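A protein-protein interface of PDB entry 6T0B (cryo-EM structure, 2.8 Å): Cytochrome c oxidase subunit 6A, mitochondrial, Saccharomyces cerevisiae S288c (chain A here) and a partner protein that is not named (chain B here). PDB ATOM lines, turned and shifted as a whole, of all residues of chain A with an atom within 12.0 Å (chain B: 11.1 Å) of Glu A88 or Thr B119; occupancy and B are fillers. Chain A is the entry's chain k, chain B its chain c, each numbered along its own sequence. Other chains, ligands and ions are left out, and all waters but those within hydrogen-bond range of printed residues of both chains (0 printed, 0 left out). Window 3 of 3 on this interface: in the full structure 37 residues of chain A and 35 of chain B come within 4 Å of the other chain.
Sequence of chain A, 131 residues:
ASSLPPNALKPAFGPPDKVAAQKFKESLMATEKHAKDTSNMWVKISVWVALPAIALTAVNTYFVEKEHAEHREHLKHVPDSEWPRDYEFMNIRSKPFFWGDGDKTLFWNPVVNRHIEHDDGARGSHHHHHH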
ATOM      1  N   PRO A  84       5.038 -29.979  10.606  1.00  0.00           N
ATOM      2  CA  PRO A  84       4.739 -28.586  10.263  1.00  0.00           C
ATOM      3  C   PRO A  84       5.289 -28.225   8.894  1.00  0.00           C
ATOM      4  O   PRO A  84       6.398 -28.617   8.527  1.00  0.00           O
ATOM      5  CB  PRO A  84       5.437 -27.792  11.371  1.00  0.00           C
ATOM      6  CG  PRO A  84       6.494 -28.685  11.853  1.00  0.00           C
ATOM      7  CD  PRO A  84       5.929 -30.062  11.772  1.00  0.00           C
ATOM      8  N   ARG A  85       4.485 -27.485   8.135  1.00  0.00           N
ATOM      9  CA  ARG A  85       4.846 -27.109   6.777  1.00  0.00           C
ATOM     10  C   ARG A  85       6.011 -26.129   6.787  1.00  0.00           C
ATOM     11  O   ARG A  85       6.047 -25.196   7.592  1.00  0.00           O
ATOM     12  CB  ARG A  85       3.636 -26.497   6.075  1.00  0.00           C
ATOM     13  CG  ARG A  85       3.870 -26.076   4.644  1.00  0.00           C
ATOM     14  CD  ARG A  85       2.606 -25.515   4.033  1.00  0.00           C
ATOM     15  NE  ARG A  85       1.585 -26.539   3.855  1.00  0.00           N
ATOM     16  CZ  ARG A  85       0.330 -26.282   3.498  1.00  0.00           C
ATOM     17  NH1 ARG A  85      -0.056 -25.028   3.288  1.00  0.00           N
ATOM     18  NH2 ARG A  85      -0.539 -27.273   3.356  1.00  0.00           N
ATOM     19  N   ASP A  86       6.977 -26.362   5.900  1.00  0.00           N
ATOM     20  CA  ASP A  86       8.183 -25.544   5.874  1.00  0.00           C
ATOM     21  C   ASP A  86       7.884 -24.137   5.380  1.00  0.00           C
ATOM     22  O   ASP A  86       7.149 -23.946   4.409  1.00  0.00           O
ATOM     23  CB  ASP A  86       9.235 -26.175   4.963  1.00  0.00           C
ATOM     24  CG  ASP A  86       9.809 -27.448   5.526  1.00  0.00           C
ATOM     25  OD1 ASP A  86       9.850 -27.589   6.767  1.00  0.00           O
ATOM     26  OD2 ASP A  86      10.231 -28.306   4.726  1.00  0.00           O
ATOM     27  N   TYR A  87       8.506 -23.152   6.024  1.00  0.00           N
ATOM     28  CA  TYR A  87       8.427 -21.774   5.571  1.00  0.00           C
ATOM     29  C   TYR A  87       9.165 -21.614   4.240  1.00  0.00           C
ATOM     30  O   TYR A  87       9.841 -22.528   3.755  1.00  0.00           O
ATOM     31  CB  TYR A  87       8.984 -20.829   6.634  1.00  0.00           C
ATOM     32  CG  TYR A  87       8.009 -20.476   7.741  1.00  0.00           C
ATOM     33  CD1 TYR A  87       7.080 -19.466   7.572  1.00  0.00           C
ATOM     34  CD2 TYR A  87       8.029 -21.144   8.958  1.00  0.00           C
ATOM     35  CE1 TYR A  87       6.187 -19.140   8.570  1.00  0.00           C
ATOM     36  CE2 TYR A  87       7.139 -20.820   9.964  1.00  0.00           C
ATOM     37  CZ  TYR A  87       6.222 -19.818   9.762  1.00  0.00           C
ATOM     38  OH  TYR A  87       5.333 -19.489  10.759  1.00  0.00           O
ATOM     39  N   GLU A  88       9.024 -20.426   3.642  1.00  0.00           N
ATOM     40  CA  GLU A  88       9.538 -20.174   2.296  1.00  0.00           C
ATOM     41  C   GLU A  88      11.053 -20.280   2.229  1.00  0.00           C
ATOM     42  O   GLU A  88      11.602 -20.786   1.244  1.00  0.00           O
ATOM     43  CB  GLU A  88       9.099 -18.787   1.830  1.00  0.00           C
ATOM     44  CG  GLU A  88       9.544 -18.431   0.426  1.00  0.00           C
ATOM     45  CD  GLU A  88       9.119 -17.046   0.010  1.00  0.00           C
ATOM     46  OE1 GLU A  88       8.521 -16.333   0.844  1.00  0.00           O
ATOM     47  OE2 GLU A  88       9.357 -16.675  -1.155  1.00  0.00           O
ATOM     48  N   PHE A  89      11.736 -19.860   3.280  1.00  0.00           N
ATOM     49  CA  PHE A  89      13.185 -19.866   3.298  1.00  0.00           C
ATOM     50  C   PHE A  89      13.774 -21.208   3.699  1.00  0.00           C
ATOM     51  O   PHE A  89      14.988 -21.387   3.578  1.00  0.00           O
ATOM     52  CB  PHE A  89      13.698 -18.769   4.238  1.00  0.00           C
ATOM     53  CG  PHE A  89      13.071 -18.780   5.602  1.00  0.00           C
ATOM     54  CD1 PHE A  89      13.631 -19.519   6.624  1.00  0.00           C
ATOM     55  CD2 PHE A  89      11.942 -18.026   5.873  1.00  0.00           C
ATOM     56  CE1 PHE A  89      13.067 -19.532   7.869  1.00  0.00           C
ATOM     57  CE2 PHE A  89      11.375 -18.038   7.120  1.00  0.00           C
ATOM     58  CZ  PHE A  89      11.941 -18.788   8.115  1.00  0.00           C
ATOM     59  N   MET A  90      12.967 -22.150   4.168  1.00  0.00           N
ATOM     60  CA  MET A  90      13.495 -23.394   4.704  1.00  0.00           C
ATOM     61  C   MET A  90      13.716 -24.404   3.590  1.00  0.00           C
ATOM     62  O   MET A  90      12.857 -24.572   2.721  1.00  0.00           O
ATOM     63  CB  MET A  90      12.552 -23.955   5.760  1.00  0.00           C
ATOM     64  CG  MET A  90      12.045 -22.901   6.710  1.00  0.00           C
ATOM     65  SD  MET A  90      11.096 -23.561   8.084  1.00  0.00           S
ATOM     66  CE  MET A  90      12.397 -24.282   9.077  1.00  0.00           C
ATOM     67  N   ASN A  91      14.878 -25.064   3.631  1.00  0.00           N
ATOM     68  CA  ASN A  91      15.315 -26.094   2.681  1.00  0.00           C
ATOM     69  C   ASN A  91      15.341 -25.558   1.248  1.00  0.00           C
ATOM     70  O   ASN A  91      14.561 -25.948   0.380  1.00  0.00           O
ATOM     71  CB  ASN A  91      14.466 -27.364   2.800  1.00  0.00           C
ATOM     72  CG  ASN A  91      14.764 -28.135   4.063  1.00  0.00           C
ATOM     73  OD1 ASN A  91      15.919 -28.272   4.461  1.00  0.00           O
ATOM     74  ND2 ASN A  91      13.722 -28.641   4.705  1.00  0.00           N
ATOM     75  N   ILE A  92      16.269 -24.620   1.050  1.00  0.00           N
ATOM     76  CA  ILE A  92      16.522 -24.050  -0.267  1.00  0.00           C
ATOM     77  C   ILE A  92      17.051 -25.127  -1.195  1.00  0.00           C
ATOM     78  O   ILE A  92      18.000 -25.847  -0.861  1.00  0.00           O
ATOM     79  CB  ILE A  92      17.515 -22.886  -0.142  1.00  0.00           C
ATOM     80  CG1 ILE A  92      16.918 -21.747   0.688  1.00  0.00           C
ATOM     81  CG2 ILE A  92      17.954 -22.393  -1.505  1.00  0.00           C
ATOM     82  CD1 ILE A  92      15.534 -21.320   0.267  1.00  0.00           C
ATOM     83  N   ARG A  93      16.420 -25.265  -2.368  1.00  0.00           N
ATOM     84  CA  ARG A  93      16.838 -26.234  -3.385  1.00  0.00           C
ATOM     85  C   ARG A  93      17.017 -25.491  -4.705  1.00  0.00           C
ATOM     86  O   ARG A  93      16.105 -25.433  -5.530  1.00  0.00           O
ATOM     87  CB  ARG A  93      15.837 -27.366  -3.508  1.00  0.00           C
ATOM     88  CG  ARG A  93      15.708 -28.202  -2.264  1.00  0.00           C
ATOM     89  CD  ARG A  93      16.993 -28.934  -1.958  1.00  0.00           C
ATOM     90  NE  ARG A  93      16.810 -29.856  -0.847  1.00  0.00           N
ATOM     91  CZ  ARG A  93      17.368 -29.706   0.344  1.00  0.00           C
ATOM     92  NH1 ARG A  93      18.164 -28.680   0.572  1.00  0.00           N
ATOM     93  NH2 ARG A  93      17.141 -30.590   1.300  1.00  0.00           N
ATOM     94  N   SER A  94      18.202 -24.922  -4.901  1.00  0.00           N
ATOM     95  CA  SER A  94      18.507 -24.256  -6.159  1.00  0.00           C
ATOM     96  C   SER A  94      18.876 -25.274  -7.229  1.00  0.00           C
ATOM     97  O   SER A  94      18.226 -25.361  -8.276  1.00  0.00           O
ATOM     98  CB  SER A  94      19.633 -23.248  -5.949  1.00  0.00           C
ATOM     99  OG  SER A  94      20.790 -23.884  -5.440  1.00  0.00           O
ATOM    100  N   ARG A 114      13.411 -33.012   7.820  1.00  0.00           N
ATOM    101  CA  ARG A 114      12.477 -33.622   6.886  1.00  0.00           C
ATOM    102  C   ARG A 114      12.105 -32.608   5.819  1.00  0.00           C
ATOM    103  O   ARG A 114      11.744 -31.473   6.141  1.00  0.00           O
ATOM    104  CB  ARG A 114      11.222 -34.120   7.607  1.00  0.00           C
ATOM    105  CG  ARG A 114      11.300 -35.570   8.065  1.00  0.00           C
ATOM    106  CD  ARG A 114      10.285 -35.868   9.145  1.00  0.00           C
ATOM    107  NE  ARG A 114      10.451 -37.208   9.683  1.00  0.00           N
ATOM    108  CZ  ARG A 114       9.744 -37.697  10.692  1.00  0.00           C
ATOM    109  NH1 ARG A 114       9.962 -38.932  11.117  1.00  0.00           N
ATOM    110  NH2 ARG A 114       8.818 -36.956  11.274  1.00  0.00           N
ATOM    111  N   HIS A 115      12.186 -33.018   4.556  1.00  0.00           N
ATOM    112  CA  HIS A 115      11.837 -32.175   3.418  1.00  0.00           C
ATOM    113  C   HIS A 115      10.687 -32.828   2.666  1.00  0.00           C
ATOM    114  O   HIS A 115      10.884 -33.829   1.971  1.00  0.00           O
ATOM    115  CB  HIS A 115      13.038 -31.975   2.501  1.00  0.00           C
ATOM    116  CG  HIS A 115      12.765 -31.079   1.336  1.00  0.00           C
ATOM    117  ND1 HIS A 115      13.327 -31.283   0.096  1.00  0.00           N
ATOM    118  CD2 HIS A 115      11.997 -29.971   1.224  1.00  0.00           C
ATOM    119  CE1 HIS A 115      12.914 -30.342  -0.731  1.00  0.00           C
ATOM    120  NE2 HIS A 115      12.105 -29.533  -0.072  1.00  0.00           N
ATOM    121  N   ILE A 116       9.495 -32.255   2.792  1.00  0.00           N
ATOM    122  CA  ILE A 116       8.291 -32.829   2.206  1.00  0.00           C
ATOM    123  C   ILE A 116       7.737 -31.933   1.104  1.00  0.00           C
ATOM    124  O   ILE A 116       7.472 -32.384  -0.012  1.00  0.00           O
ATOM    125  CB  ILE A 116       7.225 -33.079   3.282  1.00  0.00           C
ATOM    126  CG1 ILE A 116       7.709 -34.123   4.283  1.00  0.00           C
ATOM    127  CG2 ILE A 116       5.915 -33.516   2.657  1.00  0.00           C
ATOM    128  CD1 ILE A 116       8.137 -33.558   5.602  1.00  0.00           C
ATOM    129  N   SER B 112      22.819  -9.780   8.389  1.00  0.00           N
ATOM    130  CA  SER B 112      21.535 -10.457   8.370  1.00  0.00           C
ATOM    131  C   SER B 112      20.731 -10.255   9.644  1.00  0.00           C
ATOM    132  O   SER B 112      19.515 -10.446   9.619  1.00  0.00           O
ATOM    133  CB  SER B 112      21.730 -11.943   8.126  1.00  0.00           C
ATOM    134  OG  SER B 112      21.971 -12.180   6.757  1.00  0.00           O
ATOM    135  N   SER B 115      19.160  -5.681  11.168  1.00  0.00           N
ATOM    136  CA  SER B 115      17.773  -5.466  10.767  1.00  0.00           C
ATOM    137  C   SER B 115      17.475  -6.548   9.758  1.00  0.00           C
ATOM    138  O   SER B 115      17.930  -6.484   8.603  1.00  0.00           O
ATOM    139  CB  SER B 115      17.532  -4.076  10.190  1.00  0.00           C
ATOM    140  OG  SER B 115      17.480  -3.107  11.223  1.00  0.00           O
ATOM    141  N   PRO B 116      16.735  -7.585  10.144  1.00  0.00           N
ATOM    142  CA  PRO B 116      16.503  -8.713   9.249  1.00  0.00           C
ATOM    143  C   PRO B 116      15.520  -8.363   8.149  1.00  0.00           C
ATOM    144  O   PRO B 116      15.036  -7.236   8.027  1.00  0.00           O
ATOM    145  CB  PRO B 116      15.939  -9.787  10.175  1.00  0.00           C
ATOM    146  CG  PRO B 116      15.294  -9.031  11.243  1.00  0.00           C
ATOM    147  CD  PRO B 116      16.109  -7.801  11.460  1.00  0.00           C
ATOM    148  N   ASP B 117      15.210  -9.373   7.345  1.00  0.00           N
ATOM    149  CA  ASP B 117      14.351  -9.177   6.190  1.00  0.00           C
ATOM    150  C   ASP B 117      12.891  -9.055   6.563  1.00  0.00           C
ATOM    151  O   ASP B 117      12.529  -8.927   7.736  1.00  0.00           O
ATOM    152  CB  ASP B 117      14.467 -10.334   5.206  1.00  0.00           C
ATOM    153  CG  ASP B 117      15.866 -10.553   4.732  1.00  0.00           C
ATOM    154  OD1 ASP B 117      16.775  -9.826   5.178  1.00  0.00           O
ATOM    155  OD2 ASP B 117      16.054 -11.443   3.887  1.00  0.00           O
ATOM    156  N   VAL B 118      12.050  -9.081   5.535  1.00  0.00           N
ATOM    157  CA  VAL B 118      10.630  -9.307   5.706  1.00  0.00           C
ATOM    158  C   VAL B 118      10.249 -10.731   5.348  1.00  0.00           C
ATOM    159  O   VAL B 118       9.156 -11.180   5.721  1.00  0.00           O
ATOM    160  CB  VAL B 118       9.824  -8.291   4.874  1.00  0.00           C
ATOM    161  CG1 VAL B 118      10.170  -6.890   5.327  1.00  0.00           C
ATOM    162  CG2 VAL B 118      10.128  -8.457   3.402  1.00  0.00           C
ATOM    163  N   THR B 119      11.125 -11.466   4.662  1.00  0.00           N
ATOM    164  CA  THR B 119      10.833 -12.842   4.284  1.00  0.00           C
ATOM    165  C   THR B 119      11.113 -13.829   5.403  1.00  0.00           C
ATOM    166  O   THR B 119      10.680 -14.983   5.317  1.00  0.00           O
ATOM    167  CB  THR B 119      11.629 -13.241   3.039  1.00  0.00           C
ATOM    168  OG1 THR B 119      11.219 -14.544   2.617  1.00  0.00           O
ATOM    169  CG2 THR B 119      13.110 -13.250   3.316  1.00  0.00           C
ATOM    170  N   LEU B 120      11.825 -13.403   6.440  1.00  0.00           N
ATOM    171  CA  LEU B 120      11.913 -14.162   7.674  1.00  0.00           C
ATOM    172  C   LEU B 120      10.930 -13.649   8.710  1.00  0.00           C
ATOM    173  O   LEU B 120      10.512 -14.406   9.591  1.00  0.00           O
ATOM    174  CB  LEU B 120      13.335 -14.105   8.232  1.00  0.00           C
ATOM    175  CG  LEU B 120      14.494 -14.204   7.242  1.00  0.00           C
ATOM    176  CD1 LEU B 120      15.795 -14.030   7.978  1.00  0.00           C
ATOM    177  CD2 LEU B 120      14.487 -15.529   6.517  1.00  0.00           C
ATOM    178  N   GLY B 121      10.557 -12.376   8.622  1.00  0.00           N
ATOM    179  CA  GLY B 121       9.477 -11.850   9.427  1.00  0.00           C
ATOM    180  C   GLY B 121       9.844 -10.740  10.384  1.00  0.00           C
ATOM    181  O   GLY B 121       9.156 -10.564  11.396  1.00  0.00           O
ATOM    182  N   ALA B 122      10.884  -9.972  10.042  1.00  0.00           N
ATOM    183  CA  ALA B 122      11.516  -8.985  10.925  1.00  0.00           C
ATOM    184  C   ALA B 122      11.863  -9.617  12.269  1.00  0.00           C
ATOM    185  O   ALA B 122      11.549  -9.092  13.339  1.00  0.00           O
ATOM    186  CB  ALA B 122      10.645  -7.739  11.100  1.00  0.00           C
ATOM    187  N   CYS B 123      12.516 -10.770  12.195  1.00  0.00           N
ATOM    188  CA  CYS B 123      12.688 -11.649  13.336  1.00  0.00           C
ATOM    189  C   CYS B 123      14.085 -12.238  13.292  1.00  0.00           C
ATOM    190  O   CYS B 123      14.651 -12.439  12.217  1.00  0.00           O
ATOM    191  CB  CYS B 123      11.633 -12.756  13.314  1.00  0.00           C
ATOM    192  SG  CYS B 123      11.615 -13.832  14.739  1.00  0.00           S
ATOM    193  N   TRP B 124      14.644 -12.496  14.463  1.00  0.00           N
ATOM    194  CA  TRP B 124      15.905 -13.218  14.536  1.00  0.00           C
ATOM    195  C   TRP B 124      15.978 -13.983  15.849  1.00  0.00           C
ATOM    196  O   TRP B 124      15.897 -13.368  16.918  1.00  0.00           O
ATOM    197  CB  TRP B 124      17.103 -12.287  14.402  1.00  0.00           C
ATOM    198  CG  TRP B 124      18.339 -13.013  14.010  1.00  0.00           C
ATOM    199  CD1 TRP B 124      19.299 -13.492  14.837  1.00  0.00           C
ATOM    200  CD2 TRP B 124      18.744 -13.355  12.687  1.00  0.00           C
ATOM    201  NE1 TRP B 124      20.283 -14.097  14.116  1.00  0.00           N
ATOM    202  CE2 TRP B 124      19.963 -14.029  12.789  1.00  0.00           C
ATOM    203  CE3 TRP B 124      18.193 -13.149  11.425  1.00  0.00           C
ATOM    204  CZ2 TRP B 124      20.644 -14.497  11.683  1.00  0.00           C
ATOM    205  CZ3 TRP B 124      18.869 -13.620  10.330  1.00  0.00           C
ATOM    206  CH2 TRP B 124      20.081 -14.284  10.464  1.00  0.00           C
ATOM    207  N   PRO B 125      16.123 -15.316  15.829  1.00  0.00           N
ATOM    208  CA  PRO B 125      16.220 -16.265  14.722  1.00  0.00           C
ATOM    209  C   PRO B 125      14.878 -16.399  14.035  1.00  0.00           C
ATOM    210  O   PRO B 125      13.884 -16.139  14.705  1.00  0.00           O
ATOM    211  CB  PRO B 125      16.618 -17.576  15.412  1.00  0.00           C
ATOM    212  CG  PRO B 125      16.953 -17.215  16.802  1.00  0.00           C
ATOM    213  CD  PRO B 125      16.147 -16.014  17.115  1.00  0.00           C
ATOM    214  N   PRO B 126      14.856 -16.741  12.748  1.00  0.00           N
ATOM    215  CA  PRO B 126      13.611 -16.673  11.977  1.00  0.00           C
ATOM    216  C   PRO B 126      12.553 -17.635  12.485  1.00  0.00           C
ATOM    217  O   PRO B 126      12.801 -18.523  13.300  1.00  0.00           O
ATOM    218  CB  PRO B 126      14.053 -17.036  10.563  1.00  0.00           C
ATOM    219  CG  PRO B 126      15.481 -16.742  10.535  1.00  0.00           C
ATOM    220  CD  PRO B 126      16.005 -17.028  11.881  1.00  0.00           C
ATOM    221  N   VAL B 127      11.336 -17.413  11.997  1.00  0.00           N
ATOM    222  CA  VAL B 127      10.190 -18.179  12.450  1.00  0.00           C
ATOM    223  C   VAL B 127      10.318 -19.617  11.977  1.00  0.00           C
ATOM    224  O   VAL B 127      10.835 -19.895  10.889  1.00  0.00           O
ATOM    225  CB  VAL B 127       8.888 -17.517  11.966  1.00  0.00           C
ATOM    226  CG1 VAL B 127       8.742 -16.149  12.599  1.00  0.00           C
ATOM    227  CG2 VAL B 127       8.874 -17.369  10.454  1.00  0.00           C
ATOM    228  N   GLY B 128       9.926 -20.550  12.833  1.00  0.00           N
ATOM    229  CA  GLY B 128      10.093 -21.950  12.546  1.00  0.00           C
ATOM    230  C   GLY B 128      11.462 -22.517  12.841  1.00  0.00           C
ATOM    231  O   GLY B 128      11.579 -23.733  13.027  1.00  0.00           O
ATOM    232  N   ILE B 129      12.502 -21.694  12.887  1.00  0.00           N
ATOM    233  CA  ILE B 129      13.846 -22.184  13.168  1.00  0.00           C
ATOM    234  C   ILE B 129      13.973 -22.427  14.664  1.00  0.00           C
ATOM    235  O   ILE B 129      13.746 -21.522  15.472  1.00  0.00           O
ATOM    236  CB  ILE B 129      14.912 -21.200  12.677  1.00  0.00           C
ATOM    237  CG1 ILE B 129      14.964 -21.174  11.151  1.00  0.00           C
ATOM    238  CG2 ILE B 129      16.265 -21.560  13.234  1.00  0.00           C
ATOM    239  CD1 ILE B 129      15.554 -22.411  10.526  1.00  0.00           C
ATOM    240  N   SER B 197      20.681 -25.593   4.528  1.00  0.00           N
ATOM    241  CA  SER B 197      19.778 -25.140   3.490  1.00  0.00           C
ATOM    242  C   SER B 197      18.577 -24.403   4.044  1.00  0.00           C
ATOM    243  O   SER B 197      17.768 -23.893   3.265  1.00  0.00           O
ATOM    244  CB  SER B 197      19.308 -26.326   2.661  1.00  0.00           C
ATOM    245  OG  SER B 197      20.389 -26.919   1.970  1.00  0.00           O
ATOM    246  N   ASP B 198      18.444 -24.311   5.360  1.00  0.00           N
ATOM    247  CA  ASP B 198      17.263 -23.721   5.980  1.00  0.00           C
ATOM    248  C   ASP B 198      17.375 -22.212   6.092  1.00  0.00           C
ATOM    249  O   ASP B 198      17.177 -21.633   7.154  1.00  0.00           O
ATOM    250  CB  ASP B 198      17.035 -24.345   7.347  1.00  0.00           C
ATOM    251  CG  ASP B 198      16.236 -25.610   7.273  1.00  0.00           C
ATOM    252  OD1 ASP B 198      15.371 -25.709   6.383  1.00  0.00           O
ATOM    253  OD2 ASP B 198      16.466 -26.505   8.104  1.00  0.00           O
ATOM    254  N   GLY B 199      17.681 -21.564   4.992  1.00  0.00           N
ATOM    255  CA  GLY B 199      17.691 -20.134   4.979  1.00  0.00           C
ATOM    256  C   GLY B 199      19.018 -19.541   5.381  1.00  0.00           C
ATOM    257  O   GLY B 199      20.031 -20.223   5.616  1.00  0.00           O
ATOM    258  N   VAL B 200      18.987 -18.214   5.482  1.00  0.00           N
ATOM    259  CA  VAL B 200      20.195 -17.448   5.723  1.00  0.00           C
ATOM    260  C   VAL B 200      20.705 -17.682   7.135  1.00  0.00           C
ATOM    261  O   VAL B 200      21.910 -17.584   7.376  1.00  0.00           O
ATOM    262  CB  VAL B 200      19.937 -15.962   5.410  1.00  0.00           C
ATOM    263  CG1 VAL B 200      18.960 -15.347   6.383  1.00  0.00           C
ATOM    264  CG2 VAL B 200      21.224 -15.175   5.354  1.00  0.00           C
ATOM    265  N   TYR B 201      19.826 -18.077   8.060  1.00  0.00           N
ATOM    266  CA  TYR B 201      20.242 -18.379   9.420  1.00  0.00           C
ATOM    267  C   TYR B 201      21.153 -19.589   9.454  1.00  0.00           C
ATOM    268  O   TYR B 201      22.250 -19.535  10.024  1.00  0.00           O
ATOM    269  CB  TYR B 201      19.024 -18.617  10.298  1.00  0.00           C
ATOM    270  CG  TYR B 201      19.364 -18.838  11.746  1.00  0.00           C
ATOM    271  CD1 TYR B 201      19.619 -17.772  12.579  1.00  0.00           C
ATOM    272  CD2 TYR B 201      19.433 -20.109  12.278  1.00  0.00           C
ATOM    273  CE1 TYR B 201      19.936 -17.965  13.895  1.00  0.00           C
ATOM    274  CE2 TYR B 201      19.756 -20.309  13.588  1.00  0.00           C
ATOM    275  CZ  TYR B 201      20.001 -19.233  14.392  1.00  0.00           C
ATOM    276  OH  TYR B 201      20.319 -19.430  15.713  1.00  0.00           O
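The backbone carbonyl oxygen (O) of Ser B197 lies within hydrogen-bond range of the backbone NH (N) of Asn A91, 3.1 Å away. The backbone carbonyl oxygen of Ser B197 sits at hydrogen-bond distance from the backbone NH of Ile A92 (2.8 Å). The side-chain hydroxyl of Ser B197 lies within hydrogen-bond range of the guanidinium group of Arg A93 (3.2 Å). OD1 of Asp B198 is in hydrogen-bond range of N of Asn A91, 2.9 Å away. N of Gly B199 lies within hydrogen-bond range of O of Phe A89 (3.0 Å).
Glu A88 touches just one residue of chain B: Thr B119. Of the printed residues of chain B, Met A90 touches Ile B129 (3.9 Å) and Asp B198 (3.4 Å). Printed residues of chain B within 4 Å of Asn A91: Ser B197 (3.1 Å) and Asp B198 (2.9 Å). No residue of chain A comes within 4 Å of Asp B117. No residue of chain A comes within 4 Å of Val B118. Thr B119 touches just these residues of chain A: Glu A88 (3.7 Å) and Phe A89 (3.3 Å). No residue of chain A comes within 4 Å of Gly B121. Of the printed residues of chain A, Pro B126 touches Phe A89 (3.7 Å). The nearest printed residue of chain B that does not touch Glu A88 is Val B118 (7.1 Å). The nearest residue of chain A that does not touch Thr B119 is Tyr A87 (6.2 Å). The nearest printed residue of chain B that does not touch Tyr A87 is Gly B128 (4.01 Å).
N of Tyr A87 is in hydrogen-bond range of SD of Met A90, at 3.3 Å.
O of Val B127 touches CD2 of Tyr A87, at 3.6 Å. Thr B119 touches Glu A88. Thr B119 touches Phe A89. CD2 of Phe A89 touches CD2 of Leu B120 (3.6 Å). Phe A89 touches Pro B126 (CZ to CB, 3.7 Å). Val B127 touches Phe A89. Ser B197 touches Phe A89 (O to O, 3.8 Å). Phe A89 touches Asp B198 (O to C, 3.6 Å). CE of Met A90 touches CD1 of Ile B129, 3.9 Å away. OD1 of Asp B198 touches CB of Met A90 (3.4 Å).
Printed residues of chain A that touch a printed residue of chain B: Tyr A87, Glu A88, Phe A89, Met A90, Asn A91, Ile A92 and Arg A93. Hydrophobic or aromatic side chains of chain A that line the printed part of chain B: Tyr A87, Phe A89, Met A90 and Ile A92. Along chain A the printed residues that touch a printed residue of chain B span positions 87 to 93. Of the 21 printed residues of chain B, 8 touch a printed residue of chain A. Hydrophobic or aromatic side chains of chain B within 4 Å of the printed part of chain A: Leu B120, Pro B126, Val B127 and Ile B129. Among the printed residues, 15 pairs touch across the chains.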
